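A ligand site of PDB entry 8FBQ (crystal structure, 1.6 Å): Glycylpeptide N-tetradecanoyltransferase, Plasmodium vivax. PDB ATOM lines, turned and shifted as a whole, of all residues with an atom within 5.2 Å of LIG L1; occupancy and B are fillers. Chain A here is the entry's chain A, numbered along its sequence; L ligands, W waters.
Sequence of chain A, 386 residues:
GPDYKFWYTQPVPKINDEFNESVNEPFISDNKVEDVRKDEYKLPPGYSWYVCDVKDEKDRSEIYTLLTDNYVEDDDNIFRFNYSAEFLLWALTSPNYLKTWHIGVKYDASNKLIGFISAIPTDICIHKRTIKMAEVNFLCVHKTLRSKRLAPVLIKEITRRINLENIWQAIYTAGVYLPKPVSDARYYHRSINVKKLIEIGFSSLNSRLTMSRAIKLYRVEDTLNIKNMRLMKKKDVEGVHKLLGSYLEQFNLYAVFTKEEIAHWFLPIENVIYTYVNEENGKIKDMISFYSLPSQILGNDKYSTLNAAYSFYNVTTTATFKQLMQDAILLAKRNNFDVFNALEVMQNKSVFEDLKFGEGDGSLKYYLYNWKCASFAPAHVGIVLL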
ATOM      1  N   TYR A  71     -14.263  -2.956  14.615  1.00  0.00           N
ATOM      2  CA  TYR A  71     -14.969  -3.879  13.737  1.00  0.00           C
ATOM      3  C   TYR A  71     -15.725  -4.935  14.564  1.00  0.00           C
ATOM      4  O   TYR A  71     -16.089  -4.693  15.710  1.00  0.00           O
ATOM      5  CB  TYR A  71     -13.978  -4.456  12.699  1.00  0.00           C
ATOM      6  CG  TYR A  71     -14.649  -5.090  11.474  1.00  0.00           C
ATOM      7  CD1 TYR A  71     -15.664  -4.428  10.798  1.00  0.00           C
ATOM      8  CD2 TYR A  71     -14.289  -6.342  11.029  1.00  0.00           C
ATOM      9  CE1 TYR A  71     -16.295  -5.014   9.705  1.00  0.00           C
ATOM     10  CE2 TYR A  71     -14.911  -6.931   9.916  1.00  0.00           C
ATOM     11  CZ  TYR A  71     -15.908  -6.249   9.266  1.00  0.00           C
ATOM     12  OH  TYR A  71     -16.536  -6.827   8.188  1.00  0.00           O
ATOM     13  N   VAL A  72     -16.019  -6.091  13.960  1.00  0.00           N
ATOM     14  CA  VAL A  72     -17.071  -6.970  14.467  1.00  0.00           C
ATOM     15  C   VAL A  72     -16.694  -7.530  15.821  1.00  0.00           C
ATOM     16  O   VAL A  72     -15.585  -8.052  16.009  1.00  0.00           O
ATOM     17  CB  VAL A  72     -17.303  -8.113  13.465  1.00  0.00           C
ATOM     18  CG1 VAL A  72     -18.190  -9.185  14.116  1.00  0.00           C
ATOM     19  CG2 VAL A  72     -17.900  -7.610  12.169  1.00  0.00           C
ATOM     20  N   GLU A  73     -17.649  -7.504  16.755  1.00  0.00           N
ATOM     21  CA  GLU A  73     -17.528  -8.175  18.042  1.00  0.00           C
ATOM     22  C   GLU A  73     -18.605  -9.234  18.133  1.00  0.00           C
ATOM     23  O   GLU A  73     -19.663  -9.117  17.489  1.00  0.00           O
ATOM     24  CB  GLU A  73     -17.667  -7.205  19.227  1.00  0.00           C
ATOM     25  CG  GLU A  73     -16.595  -6.140  19.193  1.00  0.00           C
ATOM     26  CD  GLU A  73     -16.593  -5.204  20.380  1.00  0.00           C
ATOM     27  OE1 GLU A  73     -17.284  -5.459  21.378  1.00  0.00           O
ATOM     28  OE2 GLU A  73     -15.888  -4.168  20.299  1.00  0.00           O
ATOM     29  N   ASP A  74     -18.344 -10.296  18.895  1.00  0.00           N
ATOM     30  CA  ASP A  74     -19.398 -11.255  19.168  1.00  0.00           C
ATOM     31  C   ASP A  74     -20.464 -10.618  20.065  1.00  0.00           C
ATOM     32  O   ASP A  74     -20.293  -9.528  20.615  1.00  0.00           O
ATOM     33  CB  ASP A  74     -18.846 -12.506  19.839  1.00  0.00           C
ATOM     34  CG  ASP A  74     -18.380 -12.223  21.219  1.00  0.00           C
ATOM     35  OD1 ASP A  74     -17.450 -11.437  21.319  1.00  0.00           O
ATOM     36  OD2 ASP A  74     -18.986 -12.725  22.200  1.00  0.00           O
ATOM     37  N   PHE A  79     -14.800 -10.913  22.048  1.00  0.00           N
ATOM     38  CA  PHE A  79     -13.859 -10.973  20.938  1.00  0.00           C
ATOM     39  C   PHE A  79     -14.113  -9.833  19.971  1.00  0.00           C
ATOM     40  O   PHE A  79     -15.269  -9.435  19.769  1.00  0.00           O
ATOM     41  CB  PHE A  79     -14.024 -12.282  20.164  1.00  0.00           C
ATOM     42  CG  PHE A  79     -13.807 -13.508  20.990  1.00  0.00           C
ATOM     43  CD1 PHE A  79     -12.572 -13.770  21.515  1.00  0.00           C
ATOM     44  CD2 PHE A  79     -14.835 -14.415  21.212  1.00  0.00           C
ATOM     45  CE1 PHE A  79     -12.352 -14.890  22.282  1.00  0.00           C
ATOM     46  CE2 PHE A  79     -14.620 -15.544  21.977  1.00  0.00           C
ATOM     47  CZ  PHE A  79     -13.394 -15.791  22.516  1.00  0.00           C
ATOM     48  N   ARG A  80     -13.052  -9.349  19.333  1.00  0.00           N
ATOM     49  CA  ARG A  80     -13.168  -8.426  18.181  1.00  0.00           C
ATOM     50  C   ARG A  80     -12.263  -8.920  17.058  1.00  0.00           C
ATOM     51  O   ARG A  80     -11.091  -9.213  17.297  1.00  0.00           O
ATOM     52  CB  ARG A  80     -12.808  -6.985  18.558  1.00  0.00           C
ATOM     53  CG  ARG A  80     -13.099  -5.998  17.426  1.00  0.00           C
ATOM     54  CD  ARG A  80     -13.237  -4.538  17.921  1.00  0.00           C
ATOM     55  NE  ARG A  80     -12.088  -4.093  18.679  1.00  0.00           N
ATOM     56  CZ  ARG A  80     -12.064  -3.652  19.927  1.00  0.00           C
ATOM     57  NH1 ARG A  80     -13.158  -3.578  20.686  1.00  0.00           N
ATOM     58  NH2 ARG A  80     -10.909  -3.278  20.438  1.00  0.00           N
ATOM     59  N   PHE A  81     -12.794  -9.045  15.853  1.00  0.00           N
ATOM     60  CA  PHE A  81     -11.925  -9.496  14.762  1.00  0.00           C
ATOM     61  C   PHE A  81     -10.749  -8.542  14.620  1.00  0.00           C
ATOM     62  O   PHE A  81     -10.900  -7.331  14.770  1.00  0.00           O
ATOM     63  CB  PHE A  81     -12.662  -9.584  13.427  1.00  0.00           C
ATOM     64  CG  PHE A  81     -13.594 -10.772  13.287  1.00  0.00           C
ATOM     65  CD1 PHE A  81     -13.250 -12.026  13.783  1.00  0.00           C
ATOM     66  CD2 PHE A  81     -14.793 -10.630  12.611  1.00  0.00           C
ATOM     67  CE1 PHE A  81     -14.130 -13.102  13.636  1.00  0.00           C
ATOM     68  CE2 PHE A  81     -15.658 -11.701  12.446  1.00  0.00           C
ATOM     69  CZ  PHE A  81     -15.327 -12.928  12.976  1.00  0.00           C
ATOM     70  N   TYR A  83      -8.397  -8.534  11.664  1.00  0.00           N
ATOM     71  CA  TYR A  83      -7.841  -8.763  10.339  1.00  0.00           C
ATOM     72  C   TYR A  83      -6.498  -8.055  10.209  1.00  0.00           C
ATOM     73  O   TYR A  83      -6.389  -6.859  10.507  1.00  0.00           O
ATOM     74  CB  TYR A  83      -8.780  -8.218   9.262  1.00  0.00           C
ATOM     75  CG  TYR A  83     -10.078  -8.972   9.059  1.00  0.00           C
ATOM     76  CD1 TYR A  83     -11.193  -8.690   9.816  1.00  0.00           C
ATOM     77  CD2 TYR A  83     -10.188  -9.932   8.074  1.00  0.00           C
ATOM     78  CE1 TYR A  83     -12.385  -9.379   9.601  1.00  0.00           C
ATOM     79  CE2 TYR A  83     -11.374 -10.614   7.860  1.00  0.00           C
ATOM     80  CZ  TYR A  83     -12.461 -10.314   8.623  1.00  0.00           C
ATOM     81  OH  TYR A  83     -13.662 -10.964   8.421  1.00  0.00           O
ATOM     82  N   ASN A 137     -17.978  -5.951   2.002  1.00  0.00           N
ATOM     83  CA  ASN A 137     -17.345  -6.405   3.228  1.00  0.00           C
ATOM     84  C   ASN A 137     -16.787  -5.189   3.955  1.00  0.00           C
ATOM     85  O   ASN A 137     -16.656  -4.104   3.389  1.00  0.00           O
ATOM     86  CB  ASN A 137     -16.244  -7.417   2.910  1.00  0.00           C
ATOM     87  CG  ASN A 137     -15.917  -8.334   4.059  1.00  0.00           C
ATOM     88  OD1 ASN A 137     -16.475  -8.229   5.126  1.00  0.00           O
ATOM     89  ND2 ASN A 137     -14.997  -9.251   3.819  1.00  0.00           N
ATOM     90  N   THR A 173     -22.181 -11.281   3.724  1.00  0.00           N
ATOM     91  CA  THR A 173     -22.588 -12.055   4.888  1.00  0.00           C
ATOM     92  C   THR A 173     -22.604 -11.161   6.113  1.00  0.00           C
ATOM     93  O   THR A 173     -21.907 -10.131   6.174  1.00  0.00           O
ATOM     94  CB  THR A 173     -21.677 -13.248   5.167  1.00  0.00           C
ATOM     95  OG1 THR A 173     -20.322 -12.823   5.386  1.00  0.00           O
ATOM     96  CG2 THR A 173     -21.720 -14.211   4.014  1.00  0.00           C
ATOM     97  N   ALA A 174     -23.380 -11.578   7.110  1.00  0.00           N
ATOM     98  CA  ALA A 174     -23.376 -10.916   8.415  1.00  0.00           C
ATOM     99  C   ALA A 174     -23.804 -11.923   9.463  1.00  0.00           C
ATOM    100  O   ALA A 174     -24.590 -12.832   9.175  1.00  0.00           O
ATOM    101  CB  ALA A 174     -24.307  -9.693   8.457  1.00  0.00           C
ATOM    102  N   GLY A 175     -23.288 -11.742  10.682  1.00  0.00           N
ATOM    103  CA  GLY A 175     -23.758 -12.528  11.812  1.00  0.00           C
ATOM    104  C   GLY A 175     -25.085 -12.072  12.365  1.00  0.00           C
ATOM    105  O   GLY A 175     -25.754 -12.858  13.048  1.00  0.00           O
ATOM    106  N   TYR A 187     -22.221 -21.880  12.618  1.00  0.00           N
ATOM    107  CA  TYR A 187     -20.815 -22.206  12.639  1.00  0.00           C
ATOM    108  C   TYR A 187     -20.472 -23.135  13.797  1.00  0.00           C
ATOM    109  O   TYR A 187     -21.165 -23.188  14.819  1.00  0.00           O
ATOM    110  CB  TYR A 187     -19.935 -20.959  12.701  1.00  0.00           C
ATOM    111  CG  TYR A 187     -20.423 -19.803  13.498  1.00  0.00           C
ATOM    112  CD1 TYR A 187     -20.173 -19.725  14.865  1.00  0.00           C
ATOM    113  CD2 TYR A 187     -21.044 -18.731  12.871  1.00  0.00           C
ATOM    114  CE1 TYR A 187     -20.581 -18.621  15.589  1.00  0.00           C
ATOM    115  CE2 TYR A 187     -21.483 -17.645  13.603  1.00  0.00           C
ATOM    116  CZ  TYR A 187     -21.242 -17.596  14.960  1.00  0.00           C
ATOM    117  OH  TYR A 187     -21.658 -16.501  15.696  1.00  0.00           O
ATOM    118  N   PHE A 202     -14.228 -19.127  24.988  1.00  0.00           N
ATOM    119  CA  PHE A 202     -14.668 -19.534  23.665  1.00  0.00           C
ATOM    120  C   PHE A 202     -15.402 -20.865  23.742  1.00  0.00           C
ATOM    121  O   PHE A 202     -16.411 -21.065  23.064  1.00  0.00           O
ATOM    122  CB  PHE A 202     -13.468 -19.665  22.750  1.00  0.00           C
ATOM    123  CG  PHE A 202     -13.812 -20.075  21.358  1.00  0.00           C
ATOM    124  CD1 PHE A 202     -14.233 -19.157  20.429  1.00  0.00           C
ATOM    125  CD2 PHE A 202     -13.742 -21.415  20.993  1.00  0.00           C
ATOM    126  CE1 PHE A 202     -14.551 -19.531  19.144  1.00  0.00           C
ATOM    127  CE2 PHE A 202     -14.053 -21.792  19.702  1.00  0.00           C
ATOM    128  CZ  PHE A 202     -14.457 -20.850  18.777  1.00  0.00           C
ATOM    129  N   SER A 295      -8.934 -13.096  16.525  1.00  0.00           N
ATOM    130  CA  SER A 295      -9.791 -12.197  17.278  1.00  0.00           C
ATOM    131  C   SER A 295      -9.041 -11.712  18.504  1.00  0.00           C
ATOM    132  O   SER A 295      -8.466 -12.508  19.258  1.00  0.00           O
ATOM    133  CB  SER A 295     -11.090 -12.868  17.735  1.00  0.00           C
ATOM    134  OG  SER A 295     -11.916 -13.127  16.613  1.00  0.00           O
ATOM    135  N   LEU A 306      -7.077 -14.782  19.922  1.00  0.00           N
ATOM    136  CA  LEU A 306      -7.523 -16.102  19.520  1.00  0.00           C
ATOM    137  C   LEU A 306      -7.059 -16.338  18.090  1.00  0.00           C
ATOM    138  O   LEU A 306      -7.485 -15.625  17.180  1.00  0.00           O
ATOM    139  CB  LEU A 306      -9.037 -16.184  19.618  1.00  0.00           C
ATOM    140  CG  LEU A 306      -9.667 -17.441  19.062  1.00  0.00           C
ATOM    141  CD1 LEU A 306      -9.268 -18.641  19.887  1.00  0.00           C
ATOM    142  CD2 LEU A 306     -11.169 -17.237  19.068  1.00  0.00           C
ATOM    143  N   TYR A 310     -10.047 -20.558   9.636  1.00  0.00           N
ATOM    144  CA  TYR A 310     -11.404 -20.663   9.107  1.00  0.00           C
ATOM    145  C   TYR A 310     -11.398 -21.494   7.832  1.00  0.00           C
ATOM    146  O   TYR A 310     -10.669 -21.186   6.880  1.00  0.00           O
ATOM    147  CB  TYR A 310     -11.967 -19.272   8.801  1.00  0.00           C
ATOM    148  CG  TYR A 310     -12.330 -18.503  10.043  1.00  0.00           C
ATOM    149  CD1 TYR A 310     -11.366 -17.916  10.831  1.00  0.00           C
ATOM    150  CD2 TYR A 310     -13.641 -18.402  10.417  1.00  0.00           C
ATOM    151  CE1 TYR A 310     -11.707 -17.258  12.000  1.00  0.00           C
ATOM    152  CE2 TYR A 310     -13.986 -17.727  11.572  1.00  0.00           C
ATOM    153  CZ  TYR A 310     -13.028 -17.161  12.365  1.00  0.00           C
ATOM    154  OH  TYR A 310     -13.438 -16.504  13.521  1.00  0.00           O
ATOM    155  N   ASN A 341     -12.389 -23.278  12.635  1.00  0.00           N
ATOM    156  CA  ASN A 341     -13.801 -22.899  12.543  1.00  0.00           C
ATOM    157  C   ASN A 341     -14.337 -23.271  11.167  1.00  0.00           C
ATOM    158  O   ASN A 341     -13.641 -23.186  10.162  1.00  0.00           O
ATOM    159  CB  ASN A 341     -13.984 -21.389  12.772  1.00  0.00           C
ATOM    160  CG  ASN A 341     -13.716 -20.957  14.195  1.00  0.00           C
ATOM    161  OD1 ASN A 341     -14.018 -21.654  15.136  1.00  0.00           O
ATOM    162  ND2 ASN A 341     -13.151 -19.759  14.347  1.00  0.00           N
ATOM    163  N   ALA A 342     -15.615 -23.662  11.100  1.00  0.00           N
ATOM    164  CA  ALA A 342     -16.216 -24.043   9.820  1.00  0.00           C
ATOM    165  C   ALA A 342     -17.722 -23.789   9.906  1.00  0.00           C
ATOM    166  O   ALA A 342     -18.305 -23.779  10.987  1.00  0.00           O
ATOM    167  CB  ALA A 342     -15.975 -25.523   9.473  1.00  0.00           C
ATOM    168  N   LEU A 343     -18.323 -23.550   8.748  1.00  0.00           N
ATOM    169  CA  LEU A 343     -19.751 -23.377   8.579  1.00  0.00           C
ATOM    170  C   LEU A 343     -20.391 -24.662   8.078  1.00  0.00           C
ATOM    171  O   LEU A 343     -19.755 -25.475   7.395  1.00  0.00           O
ATOM    172  CB  LEU A 343     -19.995 -22.271   7.562  1.00  0.00           C
ATOM    173  CG  LEU A 343     -19.553 -20.866   7.974  1.00  0.00           C
ATOM    174  CD1 LEU A 343     -19.387 -19.987   6.764  1.00  0.00           C
ATOM    175  CD2 LEU A 343     -20.531 -20.279   8.972  1.00  0.00           C
ATOM    176  N   LEU A 364     -24.039 -17.584  10.600  1.00  0.00           N
ATOM    177  CA  LEU A 364     -23.644 -16.613   9.602  1.00  0.00           C
ATOM    178  C   LEU A 364     -24.698 -16.592   8.508  1.00  0.00           C
ATOM    179  O   LEU A 364     -24.979 -17.633   7.883  1.00  0.00           O
ATOM    180  CB  LEU A 364     -22.294 -16.962   9.043  1.00  0.00           C
ATOM    181  CG  LEU A 364     -21.828 -15.915   8.033  1.00  0.00           C
ATOM    182  CD1 LEU A 364     -21.374 -14.689   8.749  1.00  0.00           C
ATOM    183  CD2 LEU A 364     -20.788 -16.476   7.141  1.00  0.00           C
ATOM    184  N   LEU A 385     -17.186 -16.463   2.193  1.00  0.00           N
ATOM    185  CA  LEU A 385     -16.681 -15.106   2.146  1.00  0.00           C
ATOM    186  C   LEU A 385     -15.720 -14.870   3.306  1.00  0.00           C
ATOM    187  O   LEU A 385     -15.760 -15.571   4.325  1.00  0.00           O
ATOM    188  CB  LEU A 385     -17.815 -14.077   2.200  1.00  0.00           C
ATOM    189  CG  LEU A 385     -18.584 -13.861   0.909  1.00  0.00           C
ATOM    190  CD1 LEU A 385     -19.565 -14.995   0.712  1.00  0.00           C
ATOM    191  CD2 LEU A 385     -19.295 -12.506   0.897  1.00  0.00           C
ATOM    192  N   LEU A 386     -14.876 -13.876   3.148  1.00  0.00           N
ATOM    193  CA  LEU A 386     -13.842 -13.640   4.163  1.00  0.00           C
ATOM    194  C   LEU A 386     -14.286 -12.731   5.325  1.00  0.00           C
ATOM    195  O   LEU A 386     -15.139 -11.860   5.142  1.00  0.00           O
ATOM    196  CB  LEU A 386     -12.608 -13.080   3.466  1.00  0.00           C
ATOM    197  CG  LEU A 386     -12.027 -14.022   2.400  1.00  0.00           C
ATOM    198  CD1 LEU A 386     -11.040 -13.286   1.558  1.00  0.00           C
ATOM    199  CD2 LEU A 386     -11.374 -15.255   2.997  1.00  0.00           C
ATOM    200  OXT LEU A 386     -13.776 -12.838   6.479  1.00  0.00           O
HETATM  201  C1  LIG L   1     -17.211 -16.980  15.264  1.00  0.00           C
HETATM  202  C2  LIG L   1     -17.286 -18.319  12.864  1.00  0.00           C
HETATM  203  C3  LIG L   1     -17.223 -18.906  11.575  1.00  0.00           C
HETATM  204  C4  LIG L   1     -17.622 -18.164  10.449  1.00  0.00           C
HETATM  205  C5  LIG L   1     -18.086 -16.338  11.778  1.00  0.00           C
HETATM  206  C6  LIG L   1     -18.210 -13.936  10.929  1.00  0.00           C
HETATM  207  C7  LIG L   1     -18.754 -12.640  10.967  1.00  0.00           C
HETATM  208  N1  LIG L   1     -18.265 -11.620  10.032  1.00  0.00           N
HETATM  209  C8  LIG L   1     -19.085 -10.498   9.521  1.00  0.00           C
HETATM  210  C9  LIG L   1     -19.591 -10.896   8.114  1.00  0.00           C
HETATM  211  C10 LIG L   1     -17.701 -12.199   7.655  1.00  0.00           C
HETATM  212  C11 LIG L   1     -20.144 -13.269  12.827  1.00  0.00           C
HETATM  213  C12 LIG L   1     -19.630 -14.570  12.790  1.00  0.00           C
HETATM  214  C13 LIG L   1     -18.040 -12.864  15.912  1.00  0.00           C
HETATM  215  C14 LIG L   1     -16.723 -13.509  16.384  1.00  0.00           C
HETATM  216  C15 LIG L   1     -15.424 -11.374  16.499  1.00  0.00           C
HETATM  217  C16 LIG L   1     -15.099 -14.893  17.017  1.00  0.00           C
HETATM  218  C17 LIG L   1     -14.290 -16.153  17.382  1.00  0.00           C
HETATM  219  C18 LIG L   1     -16.445 -14.819  16.606  1.00  0.00           C
HETATM  220  C19 LIG L   1     -17.419 -16.022  16.508  1.00  0.00           C
HETATM  221  C20 LIG L   1     -17.745 -17.002  12.955  1.00  0.00           C
HETATM  222  C21 LIG L   1     -18.635 -14.884  11.830  1.00  0.00           C
HETATM  223  C22 LIG L   1     -17.144 -11.943   9.058  1.00  0.00           C
HETATM  224  C23 LIG L   1     -19.739 -12.329  11.908  1.00  0.00           C
HETATM  225  N2  LIG L   1     -15.610 -12.830  16.614  1.00  0.00           N
HETATM  226  N3  LIG L   1     -14.606 -13.677  16.991  1.00  0.00           N
HETATM  227  N4  LIG L   1     -18.027 -16.900  10.568  1.00  0.00           N
HETATM  228  N5  LIG L   1     -18.494 -11.095   7.221  1.00  0.00           N
HETATM  229  O1  LIG L   1     -17.806 -16.286  14.186  1.00  0.00           O
HETATM  230  S1  LG2 L   2     -21.122  -7.272   8.257  1.00  0.00           S
HETATM  231  C1  LG2 L   2     -20.092  -6.506   9.590  1.00  0.00           C
HETATM  232  C2  LG2 L   2     -20.689  -5.148   9.974  1.00  0.00           C
HETATM  233  N1  LG2 L   2     -19.742  -4.425  10.808  1.00  0.00           N
HETATM  234  C3  LG2 L   2     -19.641  -4.527  12.175  1.00  0.00           C
HETATM  235  O1  LG2 L   2     -20.424  -5.308  12.772  1.00  0.00           O
HETATM  236  C4  LG2 L   2     -18.583  -3.744  12.939  1.00  0.00           C
HETATM  237  C5  LG2 L   2     -19.012  -3.147  14.241  1.00  0.00           C
HETATM  238  N2  LG2 L   2     -20.256  -2.410  14.095  1.00  0.00           N
HETATM  239  C6  LG2 L   2     -20.354  -1.236  13.389  1.00  0.00           C
HETATM  240  O2  LG2 L   2     -19.324  -0.761  12.853  1.00  0.00           O
HETATM  241  C7  LG2 L   2     -21.710  -0.534  13.315  1.00  0.00           C
HETATM  242  O3  LG2 L   2     -22.483  -1.040  14.401  1.00  0.00           O
HETATM  243  C8  LG2 L   2     -22.397  -0.795  11.945  1.00  0.00           C
HETATM  244  C9  LG2 L   2     -23.760  -0.081  11.971  1.00  0.00           C
HETATM  245  C10 LG2 L   2     -22.598  -2.290  11.703  1.00  0.00           C
HETATM  246  C11 LG2 L   2     -21.552  -0.207  10.811  1.00  0.00           C
HETATM  247  N3  LG2 L   2     -25.027  -4.831   7.841  1.00  0.00           N
HETATM  248  O4  LG2 L   2     -27.187   4.315  12.950  1.00  0.00           O
HETATM  249  P1  LG2 L   2     -26.301   3.420  12.130  1.00  0.00           P
HETATM  250  C12 LG2 L   2     -28.256  -1.298   9.868  1.00  0.00           C
HETATM  251  C13 LG2 L   2     -25.938  -3.991   7.280  1.00  0.00           C
HETATM  252  O5  LG2 L   2     -25.190   4.018  11.333  1.00  0.00           O
HETATM  253  P2  LG2 L   2     -24.325   1.900  13.634  1.00  0.00           P
HETATM  254  C14 LG2 L   2     -20.525  -6.528   6.738  1.00  0.00           C
HETATM  255  O6  LG2 L   2     -19.552  -5.808   6.764  1.00  0.00           O
HETATM  256  C15 LG2 L   2     -29.437  -1.332  10.822  1.00  0.00           C
HETATM  257  O7  LG2 L   2     -30.357  -2.260  10.307  1.00  0.00           O
HETATM  258  N4  LG2 L   2     -26.736  -3.081   7.879  1.00  0.00           N
HETATM  259  O8  LG2 L   2     -25.741   2.172  13.040  1.00  0.00           O
HETATM  260  C16 LG2 L   2     -21.302  -6.722   5.470  1.00  0.00           C
HETATM  261  C17 LG2 L   2     -30.024   0.108  10.607  1.00  0.00           C
HETATM  262  O9  LG2 L   2     -30.835   0.141   9.559  1.00  0.00           O
HETATM  263  P3  LG2 L   2     -32.579  -0.056   9.803  1.00  0.00           P
HETATM  264  C18 LG2 L   2     -26.595  -3.063   9.238  1.00  0.00           C
HETATM  265  O10 LG2 L   2     -23.647   3.194  13.927  1.00  0.00           O
HETATM  266  C19 LG2 L   2     -22.063  -5.429   5.223  1.00  0.00           C
HETATM  267  C20 LG2 L   2     -28.710   0.931  10.340  1.00  0.00           C
HETATM  268  O11 LG2 L   2     -27.656  -0.041  10.109  1.00  0.00           O
HETATM  269  C21 LG2 L   2     -25.696  -3.909   9.955  1.00  0.00           C
HETATM  270  O12 LG2 L   2     -24.397   0.837  14.702  1.00  0.00           O
HETATM  271  C22 LG2 L   2     -23.113  -5.412   4.202  1.00  0.00           C
HETATM  272  C23 LG2 L   2     -28.280   1.806  11.503  1.00  0.00           C
HETATM  273  O13 LG2 L   2     -27.259   2.657  11.076  1.00  0.00           O
HETATM  274  C24 LG2 L   2     -24.913  -4.818   9.187  1.00  0.00           C
HETATM  275  N5  LG2 L   2     -24.023  -5.664   9.795  1.00  0.00           N
HETATM  276  O14 LG2 L   2     -23.541   1.232  12.295  1.00  0.00           O
HETATM  277  C25 LG2 L   2     -23.735  -4.008   4.051  1.00  0.00           C
HETATM  278  N6  LG2 L   2     -25.817  -3.675  11.340  1.00  0.00           N
HETATM  279  O15 LG2 L   2     -32.690  -1.121  10.893  1.00  0.00           O
HETATM  280  C26 LG2 L   2     -24.945  -4.036   3.135  1.00  0.00           C
HETATM  281  C27 LG2 L   2     -26.728  -2.690  11.433  1.00  0.00           C
HETATM  282  O16 LG2 L   2     -33.028   1.318  10.302  1.00  0.00           O
HETATM  283  C28 LG2 L   2     -24.559  -4.073   1.693  1.00  0.00           C
HETATM  284  N7  LG2 L   2     -27.231  -2.317  10.177  1.00  0.00           N
HETATM  285  O17 LG2 L   2     -33.046  -0.511   8.444  1.00  0.00           O
HETATM  286  C29 LG2 L   2     -25.692  -4.026   0.673  1.00  0.00           C
HETATM  287  C30 LG2 L   2     -25.224  -4.032  -0.774  1.00  0.00           C
HETATM  288  C31 LG2 L   2     -24.673  -2.681  -1.259  1.00  0.00           C
HETATM  289  C32 LG2 L   2     -24.107  -2.710  -2.660  1.00  0.00           C
HETATM  290  C33 LG2 L   2     -25.191  -2.942  -3.720  1.00  0.00           C
HETATM  291  C34 LG2 L   2     -24.678  -2.968  -5.152  1.00  0.00           C
HETATM  292  C35 LG2 L   2     -25.742  -3.240  -6.196  1.00  0.00           C
HETATM  293  O   HOH W   1     -17.358 -15.814   8.021  1.00  0.00           O
HETATM  294  O   HOH W   2     -17.810 -11.646   4.637  1.00  0.00           O
HETATM  295  O   HOH W   3     -16.801 -21.303  14.617  1.00  0.00           O
HETATM  296  O   HOH W   4     -15.686  -9.306   7.505  1.00  0.00           O
HETATM  297  O   HOH W   5     -18.454 -14.863   5.724  1.00  0.00           O
HETATM  298  O   HOH W   6     -18.904  -8.976   6.011  1.00  0.00           O
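OG of Ser 295 sits at hydrogen-bond distance from N3 of LIG L1 (2.8 Å).
A nitrogen (N5) of LIG L1 is in hydrogen-bond range of the side-chain hydroxyl (OG1) of Thr 173.
OH of Tyr 71 is in hydrogen-bond range of O6 of LG2 L2.
Water W2 lies within hydrogen-bond range of O of Leu 386, N5 of LIG L1 and OG1 of Thr 173.
Water W4 lies within hydrogen-bond range of the side-chain hydroxyl (OH) of Tyr 71 (2.7 Å), the side-chain amide oxygen (OD1) of Asn 137 (2.7 Å), the side-chain hydroxyl (OH) of Tyr 83 (2.8 Å) and a nitrogen (N5) of LIG L1 (3.3 Å).
Water W5 bridges the side-chain hydroxyl (OG1) of Thr 173 (2.8 Å) and the backbone carbonyl oxygen (O) of Leu 385 (3.1 Å).
The backbone NH of Leu 306 is in hydrogen-bond range of the backbone carbonyl oxygen of Ser 295 (2.7 Å).
The backbone NH (N) of Phe 81 is in hydrogen-bond range of the backbone carbonyl oxygen (O) of Val 72, 3.0 Å away.
The side-chain hydroxyl of Tyr 310 sits close to the side-chain amide nitrogen of Asn 341 (3.4 Å).
The side-chain carboxylate (OD1) of Asp 74 lies within hydrogen-bond range of the backbone NH (N) of Phe 79 (2.8 Å).
The side-chain hydroxyl of Tyr 83 is in hydrogen-bond range of the chain-end carboxylate of Leu 386, 2.7 Å away.
The chain-end carboxylate of Leu 386 is in hydrogen-bond range of the side-chain amide nitrogen of Asn 137 (2.9 Å).
O of Val 72 touches C15 of LIG L1, 3.4 Å away.
Asp 74 touches LIG L1.
CB of Phe 79 touches N3 of LIG L1, 3.5 Å away.
CE1 of Phe 81 touches N2 of LIG L1 (3.3 Å).
Tyr 83 touches LIG L1.
Ala 174 touches LIG L1 (CA to C9, 3.8 Å).
N of Gly 175 touches C23 of LIG L1 (3.8 Å).
CG of Tyr 187 touches C2 of LIG L1, 3.5 Å away.
Phe 202 touches LIG L1.
Leu 306 touches LIG L1.
CE2 of Tyr 310 touches C3 of LIG L1, 3.4 Å away.
Leu 343 touches LIG L1.
Leu 364 touches LIG L1.
O of Leu 386 touches C10 of LIG L1, 3.6 Å away.
Hydrophobic or aromatic side chains within 4 Å of LIG L1: Phe 79, Phe 81, Tyr 187, Phe 202, Leu 306, Tyr 310, Leu 343 and Leu 364.
Of the 23 residues printed, 16 come within 4 Å of LIG L1.
The nearest printed residue that does not touch LIG L1 is Arg 80 (4.04 Å).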
